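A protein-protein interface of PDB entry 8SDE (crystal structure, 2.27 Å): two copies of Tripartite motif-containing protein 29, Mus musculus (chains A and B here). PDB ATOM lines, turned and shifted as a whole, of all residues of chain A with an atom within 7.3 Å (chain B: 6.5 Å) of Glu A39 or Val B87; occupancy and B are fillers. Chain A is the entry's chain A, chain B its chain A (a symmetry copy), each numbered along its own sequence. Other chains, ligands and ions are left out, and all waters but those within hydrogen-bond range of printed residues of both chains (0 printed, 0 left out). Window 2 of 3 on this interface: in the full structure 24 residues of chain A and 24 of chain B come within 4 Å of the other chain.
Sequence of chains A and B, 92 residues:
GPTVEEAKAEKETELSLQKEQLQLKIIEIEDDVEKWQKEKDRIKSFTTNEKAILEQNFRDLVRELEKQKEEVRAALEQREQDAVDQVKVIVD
The indole nitrogen of Trp A36 sits close to the backbone carbonyl oxygen of Val B87 (3.3 Å).
Of the 13 printed residues of chain A, 3 touch a printed residue of chain B. Printed residues of chain A that touch a printed residue of chain B: Trp A36, Glu A39 and Ile A43. Hydrophobic or aromatic side chains of chain A that line the printed part of chain B: Trp A36 and Ile A43. Of the 8 printed residues of chain B, 5 touch a printed residue of chain A. Hydrophobic or aromatic side chains of chain B that line the printed part of chain A: Val B84, Val B87 and Val B89. Among the printed residues, 6 pairs touch across the chains.
Glu A39 touches just one residue of chain B: Val B87 (3.7 Å). Of the printed residues of chain B, Ile A43 touches Ala B83 (3.9 Å) and Val B84 (3.99 Å). Of the printed residues of chain A, Ala B83 touches Ile A43 (3.9 Å). Of the printed residues of chain A, Val B84 touches Ile A43 (3.99 Å). Val B87 touches just these residues of chain A: Trp A36 (3.3 Å) and Glu A39 (3.7 Å). The nearest residue of chain A that does not touch Val B87 is Ile A43 (4.6 Å).
OE2 of Glu A39 is in salt-bridge range of NH1 of Arg A42, at 2.9 Å.
Trp A36 touches Lys B88 (CD1 to O, 3.3 Å). Trp A36 touches Val B89 (CD2 to CG2, 3.4 Å). Val B87 touches Glu A39. Ile A43 touches Ala B83. Val B84 touches Ile A43.
No position is printed for both chains. Of the 6 pairs that touch across the chains among the printed residues, none has its exchanged pair printed and touching as well.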
ATOM      1  N   VAL A  33      19.394 -18.770  14.900  1.00  0.00           N
ATOM      2  CA  VAL A  33      19.615 -19.338  13.575  1.00  0.00           C
ATOM      3  C   VAL A  33      20.384 -20.660  13.651  1.00  0.00           C
ATOM      4  O   VAL A  33      20.071 -21.608  12.932  1.00  0.00           O
ATOM      5  CB  VAL A  33      20.307 -18.324  12.640  1.00  0.00           C
ATOM      6  CG1 VAL A  33      20.932 -18.967  11.406  1.00  0.00           C
ATOM      7  CG2 VAL A  33      19.376 -17.183  12.280  1.00  0.00           C
ATOM      8  N   GLU A  34      21.408 -20.743  14.495  1.00  0.00           N
ATOM      9  CA  GLU A  34      22.176 -21.983  14.575  1.00  0.00           C
ATOM     10  C   GLU A  34      21.310 -23.087  15.211  1.00  0.00           C
ATOM     11  O   GLU A  34      21.329 -24.265  14.829  1.00  0.00           O
ATOM     12  CB  GLU A  34      23.510 -21.685  15.246  1.00  0.00           C
ATOM     13  CG  GLU A  34      24.418 -22.873  15.492  1.00  0.00           C
ATOM     14  CD  GLU A  34      25.793 -22.519  16.081  1.00  0.00           C
ATOM     15  OE1 GLU A  34      26.709 -23.387  16.039  1.00  0.00           O
ATOM     16  OE2 GLU A  34      25.965 -21.370  16.573  1.00  0.00           O
ATOM     17  N   LYS A  35      20.464 -22.692  16.146  1.00  0.00           N
ATOM     18  CA  LYS A  35      19.607 -23.663  16.809  1.00  0.00           C
ATOM     19  C   LYS A  35      18.520 -24.153  15.824  1.00  0.00           C
ATOM     20  O   LYS A  35      18.211 -25.342  15.760  1.00  0.00           O
ATOM     21  CB  LYS A  35      19.044 -22.915  18.018  1.00  0.00           C
ATOM     22  CG  LYS A  35      17.812 -23.526  18.669  1.00  0.00           C
ATOM     23  CD  LYS A  35      17.558 -22.929  20.050  1.00  0.00           C
ATOM     24  CE  LYS A  35      16.517 -23.681  20.854  1.00  0.00           C
ATOM     25  NZ  LYS A  35      16.789 -23.601  22.310  1.00  0.00           N
ATOM     26  N   TRP A  36      17.973 -23.234  15.005  1.00  0.00           N
ATOM     27  CA  TRP A  36      16.962 -23.569  14.004  1.00  0.00           C
ATOM     28  C   TRP A  36      17.523 -24.648  13.085  1.00  0.00           C
ATOM     29  O   TRP A  36      16.973 -25.753  12.921  1.00  0.00           O
ATOM     30  CB  TRP A  36      16.518 -22.316  13.234  1.00  0.00           C
ATOM     31  CG  TRP A  36      15.716 -22.560  11.983  1.00  0.00           C
ATOM     32  CD1 TRP A  36      14.485 -23.147  11.890  1.00  0.00           C
ATOM     33  CD2 TRP A  36      16.075 -22.191  10.634  1.00  0.00           C
ATOM     34  NE1 TRP A  36      14.065 -23.187  10.588  1.00  0.00           N
ATOM     35  CE2 TRP A  36      15.016 -22.604   9.794  1.00  0.00           C
ATOM     36  CE3 TRP A  36      17.184 -21.558  10.051  1.00  0.00           C
ATOM     37  CZ2 TRP A  36      15.036 -22.399   8.414  1.00  0.00           C
ATOM     38  CZ3 TRP A  36      17.206 -21.364   8.685  1.00  0.00           C
ATOM     39  CH2 TRP A  36      16.144 -21.776   7.878  1.00  0.00           C
ATOM     40  N   GLN A  37      18.725 -24.346  12.610  1.00  0.00           N
ATOM     41  CA  GLN A  37      19.399 -25.133  11.601  1.00  0.00           C
ATOM     42  C   GLN A  37      19.799 -26.503  12.146  1.00  0.00           C
ATOM     43  O   GLN A  37      19.702 -27.515  11.433  1.00  0.00           O
ATOM     44  CB  GLN A  37      20.568 -24.287  11.072  1.00  0.00           C
ATOM     45  CG  GLN A  37      21.758 -25.130  10.630  1.00  0.00           C
ATOM     46  CD  GLN A  37      21.605 -25.501   9.173  1.00  0.00           C
ATOM     47  OE1 GLN A  37      20.598 -25.182   8.525  1.00  0.00           O
ATOM     48  NE2 GLN A  37      22.615 -26.184   8.652  1.00  0.00           N
ATOM     49  N   LYS A  38      20.283 -26.536  13.400  1.00  0.00           N
ATOM     50  CA  LYS A  38      20.597 -27.804  14.029  1.00  0.00           C
ATOM     51  C   LYS A  38      19.325 -28.644  14.208  1.00  0.00           C
ATOM     52  O   LYS A  38      19.366 -29.854  14.064  1.00  0.00           O
ATOM     53  CB  LYS A  38      21.305 -27.560  15.368  1.00  0.00           C
ATOM     54  CG  LYS A  38      21.111 -28.641  16.420  1.00  0.00           C
ATOM     55  CD  LYS A  38      22.153 -28.713  17.533  1.00  0.00           C
ATOM     56  CE  LYS A  38      21.687 -29.608  18.675  1.00  0.00           C
ATOM     57  NZ  LYS A  38      22.792 -30.329  19.363  1.00  0.00           N
ATOM     58  N   GLU A  39      18.190 -28.033  14.558  1.00  0.00           N
ATOM     59  CA  GLU A  39      16.969 -28.836  14.702  1.00  0.00           C
ATOM     60  C   GLU A  39      16.521 -29.422  13.350  1.00  0.00           C
ATOM     61  O   GLU A  39      16.194 -30.601  13.239  1.00  0.00           O
ATOM     62  CB  GLU A  39      15.819 -27.979  15.247  1.00  0.00           C
ATOM     63  CG  GLU A  39      14.535 -28.755  15.439  1.00  0.00           C
ATOM     64  CD  GLU A  39      14.691 -29.904  16.428  1.00  0.00           C
ATOM     65  OE1 GLU A  39      15.653 -29.869  17.236  1.00  0.00           O
ATOM     66  OE2 GLU A  39      13.848 -30.823  16.404  1.00  0.00           O
ATOM     67  N   LYS A  40      16.462 -28.588  12.306  1.00  0.00           N
ATOM     68  CA  LYS A  40      16.114 -29.044  10.962  1.00  0.00           C
ATOM     69  C   LYS A  40      16.970 -30.254  10.571  1.00  0.00           C
ATOM     70  O   LYS A  40      16.458 -31.254  10.078  1.00  0.00           O
ATOM     71  CB  LYS A  40      16.241 -27.876   9.979  1.00  0.00           C
ATOM     72  CG  LYS A  40      16.794 -28.196   8.599  1.00  0.00           C
ATOM     73  CD  LYS A  40      16.289 -27.269   7.490  1.00  0.00           C
ATOM     74  CE  LYS A  40      16.194 -25.813   7.891  1.00  0.00           C
ATOM     75  NZ  LYS A  40      16.545 -24.925   6.758  1.00  0.00           N
ATOM     76  N   ASP A  41      18.271 -30.178  10.837  1.00  0.00           N
ATOM     77  CA  ASP A  41      19.244 -31.200  10.489  1.00  0.00           C
ATOM     78  C   ASP A  41      19.009 -32.458  11.322  1.00  0.00           C
ATOM     79  O   ASP A  41      19.308 -33.564  10.882  1.00  0.00           O
ATOM     80  CB  ASP A  41      20.679 -30.752  10.843  1.00  0.00           C
ATOM     81  CG  ASP A  41      21.393 -29.920   9.782  1.00  0.00           C
ATOM     82  OD1 ASP A  41      20.717 -29.472   8.826  1.00  0.00           O
ATOM     83  OD2 ASP A  41      22.631 -29.702   9.922  1.00  0.00           O
ATOM     84  N   ARG A  42      18.544 -32.278  12.559  1.00  0.00           N
ATOM     85  CA  ARG A  42      18.328 -33.425  13.423  1.00  0.00           C
ATOM     86  C   ARG A  42      17.119 -34.218  12.913  1.00  0.00           C
ATOM     87  O   ARG A  42      17.138 -35.434  12.939  1.00  0.00           O
ATOM     88  CB  ARG A  42      18.151 -32.934  14.870  1.00  0.00           C
ATOM     89  CG  ARG A  42      18.066 -34.081  15.884  1.00  0.00           C
ATOM     90  CD  ARG A  42      17.362 -33.716  17.202  1.00  0.00           C
ATOM     91  NE  ARG A  42      15.995 -33.326  16.854  1.00  0.00           N
ATOM     92  CZ  ARG A  42      14.956 -34.165  16.697  1.00  0.00           C
ATOM     93  NH1 ARG A  42      13.766 -33.702  16.334  1.00  0.00           N
ATOM     94  NH2 ARG A  42      15.107 -35.464  16.902  1.00  0.00           N
ATOM     95  N   ILE A  43      16.067 -33.523  12.462  1.00  0.00           N
ATOM     96  CA  ILE A  43      14.831 -34.151  12.015  1.00  0.00           C
ATOM     97  C   ILE A  43      15.121 -34.910  10.721  1.00  0.00           C
ATOM     98  O   ILE A  43      14.676 -36.043  10.541  1.00  0.00           O
ATOM     99  CB  ILE A  43      13.759 -33.062  11.774  1.00  0.00           C
ATOM    100  CG1 ILE A  43      13.333 -32.351  13.057  1.00  0.00           C
ATOM    101  CG2 ILE A  43      12.566 -33.596  10.997  1.00  0.00           C
ATOM    102  CD1 ILE A  43      12.475 -31.097  12.792  1.00  0.00           C
ATOM    103  N   LYS A  44      15.879 -34.270   9.827  1.00  0.00           N
ATOM    104  CA  LYS A  44      16.343 -34.915   8.599  1.00  0.00           C
ATOM    105  C   LYS A  44      17.127 -36.178   8.902  1.00  0.00           C
ATOM    106  O   LYS A  44      17.071 -37.200   8.197  1.00  0.00           O
ATOM    107  CB  LYS A  44      17.257 -33.983   7.786  1.00  0.00           C
ATOM    108  CG  LYS A  44      16.509 -32.992   6.899  1.00  0.00           C
ATOM    109  CD  LYS A  44      17.341 -32.342   5.788  1.00  0.00           C
ATOM    110  CE  LYS A  44      16.506 -31.496   4.844  1.00  0.00           C
ATOM    111  NZ  LYS A  44      17.319 -30.523   4.072  1.00  0.00           N
ATOM    112  N   SER A  45      17.956 -36.077   9.935  1.00  0.00           N
ATOM    113  CA  SER A  45      18.819 -37.183  10.266  1.00  0.00           C
ATOM    114  C   SER A  45      17.961 -38.319  10.840  1.00  0.00           C
ATOM    115  O   SER A  45      18.201 -39.493  10.581  1.00  0.00           O
ATOM    116  CB  SER A  45      19.882 -36.693  11.205  1.00  0.00           C
ATOM    117  OG  SER A  45      20.821 -37.728  11.478  1.00  0.00           O
ATOM    118  N   ASP B  82       6.635 -31.511   7.249  1.00  0.00           N
ATOM    119  CA  ASP B  82       5.729 -30.908   8.215  1.00  0.00           C
ATOM    120  C   ASP B  82       6.516 -30.406   9.420  1.00  0.00           C
ATOM    121  O   ASP B  82       6.240 -29.320   9.920  1.00  0.00           O
ATOM    122  CB  ASP B  82       4.604 -31.844   8.673  1.00  0.00           C
ATOM    123  CG  ASP B  82       3.397 -31.877   7.738  1.00  0.00           C
ATOM    124  OD1 ASP B  82       3.583 -31.634   6.520  1.00  0.00           O
ATOM    125  OD2 ASP B  82       2.273 -32.154   8.228  1.00  0.00           O
ATOM    126  N   ALA B  83       7.486 -31.204   9.878  1.00  0.00           N
ATOM    127  CA  ALA B  83       8.141 -30.908  11.142  1.00  0.00           C
ATOM    128  C   ALA B  83       9.177 -29.800  10.944  1.00  0.00           C
ATOM    129  O   ALA B  83       9.340 -28.939  11.807  1.00  0.00           O
ATOM    130  CB  ALA B  83       8.742 -32.156  11.732  1.00  0.00           C
ATOM    131  N   VAL B  84       9.834 -29.823   9.782  1.00  0.00           N
ATOM    132  CA  VAL B  84      10.843 -28.858   9.390  1.00  0.00           C
ATOM    133  C   VAL B  84      10.218 -27.460   9.240  1.00  0.00           C
ATOM    134  O   VAL B  84      10.858 -26.456   9.553  1.00  0.00           O
ATOM    135  CB  VAL B  84      11.622 -29.391   8.162  1.00  0.00           C
ATOM    136  CG1 VAL B  84      12.284 -28.316   7.315  1.00  0.00           C
ATOM    137  CG2 VAL B  84      12.663 -30.422   8.579  1.00  0.00           C
ATOM    138  N   ASP B  85       8.943 -27.394   8.830  1.00  0.00           N
ATOM    139  CA  ASP B  85       8.219 -26.137   8.727  1.00  0.00           C
ATOM    140  C   ASP B  85       7.672 -25.697  10.084  1.00  0.00           C
ATOM    141  O   ASP B  85       7.359 -24.526  10.274  1.00  0.00           O
ATOM    142  CB  ASP B  85       7.058 -26.258   7.741  1.00  0.00           C
ATOM    143  CG  ASP B  85       7.511 -26.657   6.352  1.00  0.00           C
ATOM    144  OD1 ASP B  85       8.743 -26.739   6.132  1.00  0.00           O
ATOM    145  OD2 ASP B  85       6.630 -26.892   5.505  1.00  0.00           O
ATOM    146  N   GLN B  86       7.545 -26.640  11.019  1.00  0.00           N
ATOM    147  CA  GLN B  86       7.013 -26.366  12.346  1.00  0.00           C
ATOM    148  C   GLN B  86       8.110 -25.848  13.288  1.00  0.00           C
ATOM    149  O   GLN B  86       7.802 -25.444  14.413  1.00  0.00           O
ATOM    150  CB  GLN B  86       6.359 -27.642  12.886  1.00  0.00           C
ATOM    151  CG  GLN B  86       5.325 -27.432  13.986  1.00  0.00           C
ATOM    152  CD  GLN B  86       5.031 -28.718  14.721  1.00  0.00           C
ATOM    153  OE1 GLN B  86       3.995 -29.348  14.515  1.00  0.00           O
ATOM    154  NE2 GLN B  86       5.953 -29.134  15.578  1.00  0.00           N
ATOM    155  N   VAL B  87       9.382 -25.872  12.840  1.00  0.00           N
ATOM    156  CA  VAL B  87      10.510 -25.399  13.643  1.00  0.00           C
ATOM    157  C   VAL B  87      10.767 -23.922  13.347  1.00  0.00           C
ATOM    158  O   VAL B  87      11.196 -23.558  12.247  1.00  0.00           O
ATOM    159  CB  VAL B  87      11.796 -26.259  13.550  1.00  0.00           C
ATOM    160  CG1 VAL B  87      12.231 -26.564  12.124  1.00  0.00           C
ATOM    161  CG2 VAL B  87      12.953 -25.636  14.317  1.00  0.00           C
ATOM    162  N   LYS B  88      10.489 -23.092  14.363  1.00  0.00           N
ATOM    163  CA  LYS B  88      10.533 -21.640  14.260  1.00  0.00           C
ATOM    164  C   LYS B  88      11.977 -21.135  14.198  1.00  0.00           C
ATOM    165  O   LYS B  88      12.913 -21.860  14.536  1.00  0.00           O
ATOM    166  CB  LYS B  88       9.735 -21.018  15.412  1.00  0.00           C
ATOM    167  CG  LYS B  88       8.293 -20.660  15.080  1.00  0.00           C
ATOM    168  CD  LYS B  88       7.418 -21.857  14.763  1.00  0.00           C
ATOM    169  CE  LYS B  88       6.218 -21.498  13.905  1.00  0.00           C
ATOM    170  NZ  LYS B  88       5.493 -22.715  13.459  1.00  0.00           N
ATOM    171  N   VAL B  89      12.146 -19.882  13.751  1.00  0.00           N
ATOM    172  CA  VAL B  89      13.445 -19.224  13.787  1.00  0.00           C
ATOM    173  C   VAL B  89      13.599 -18.421  15.084  1.00  0.00           C
ATOM    174  O   VAL B  89      14.727 -18.180  15.513  1.00  0.00           O
ATOM    175  CB  VAL B  89      13.739 -18.422  12.500  1.00  0.00           C
ATOM    176  CG1 VAL B  89      14.285 -17.027  12.767  1.00  0.00           C
ATOM    177  CG2 VAL B  89      14.684 -19.190  11.591  1.00  0.00           C
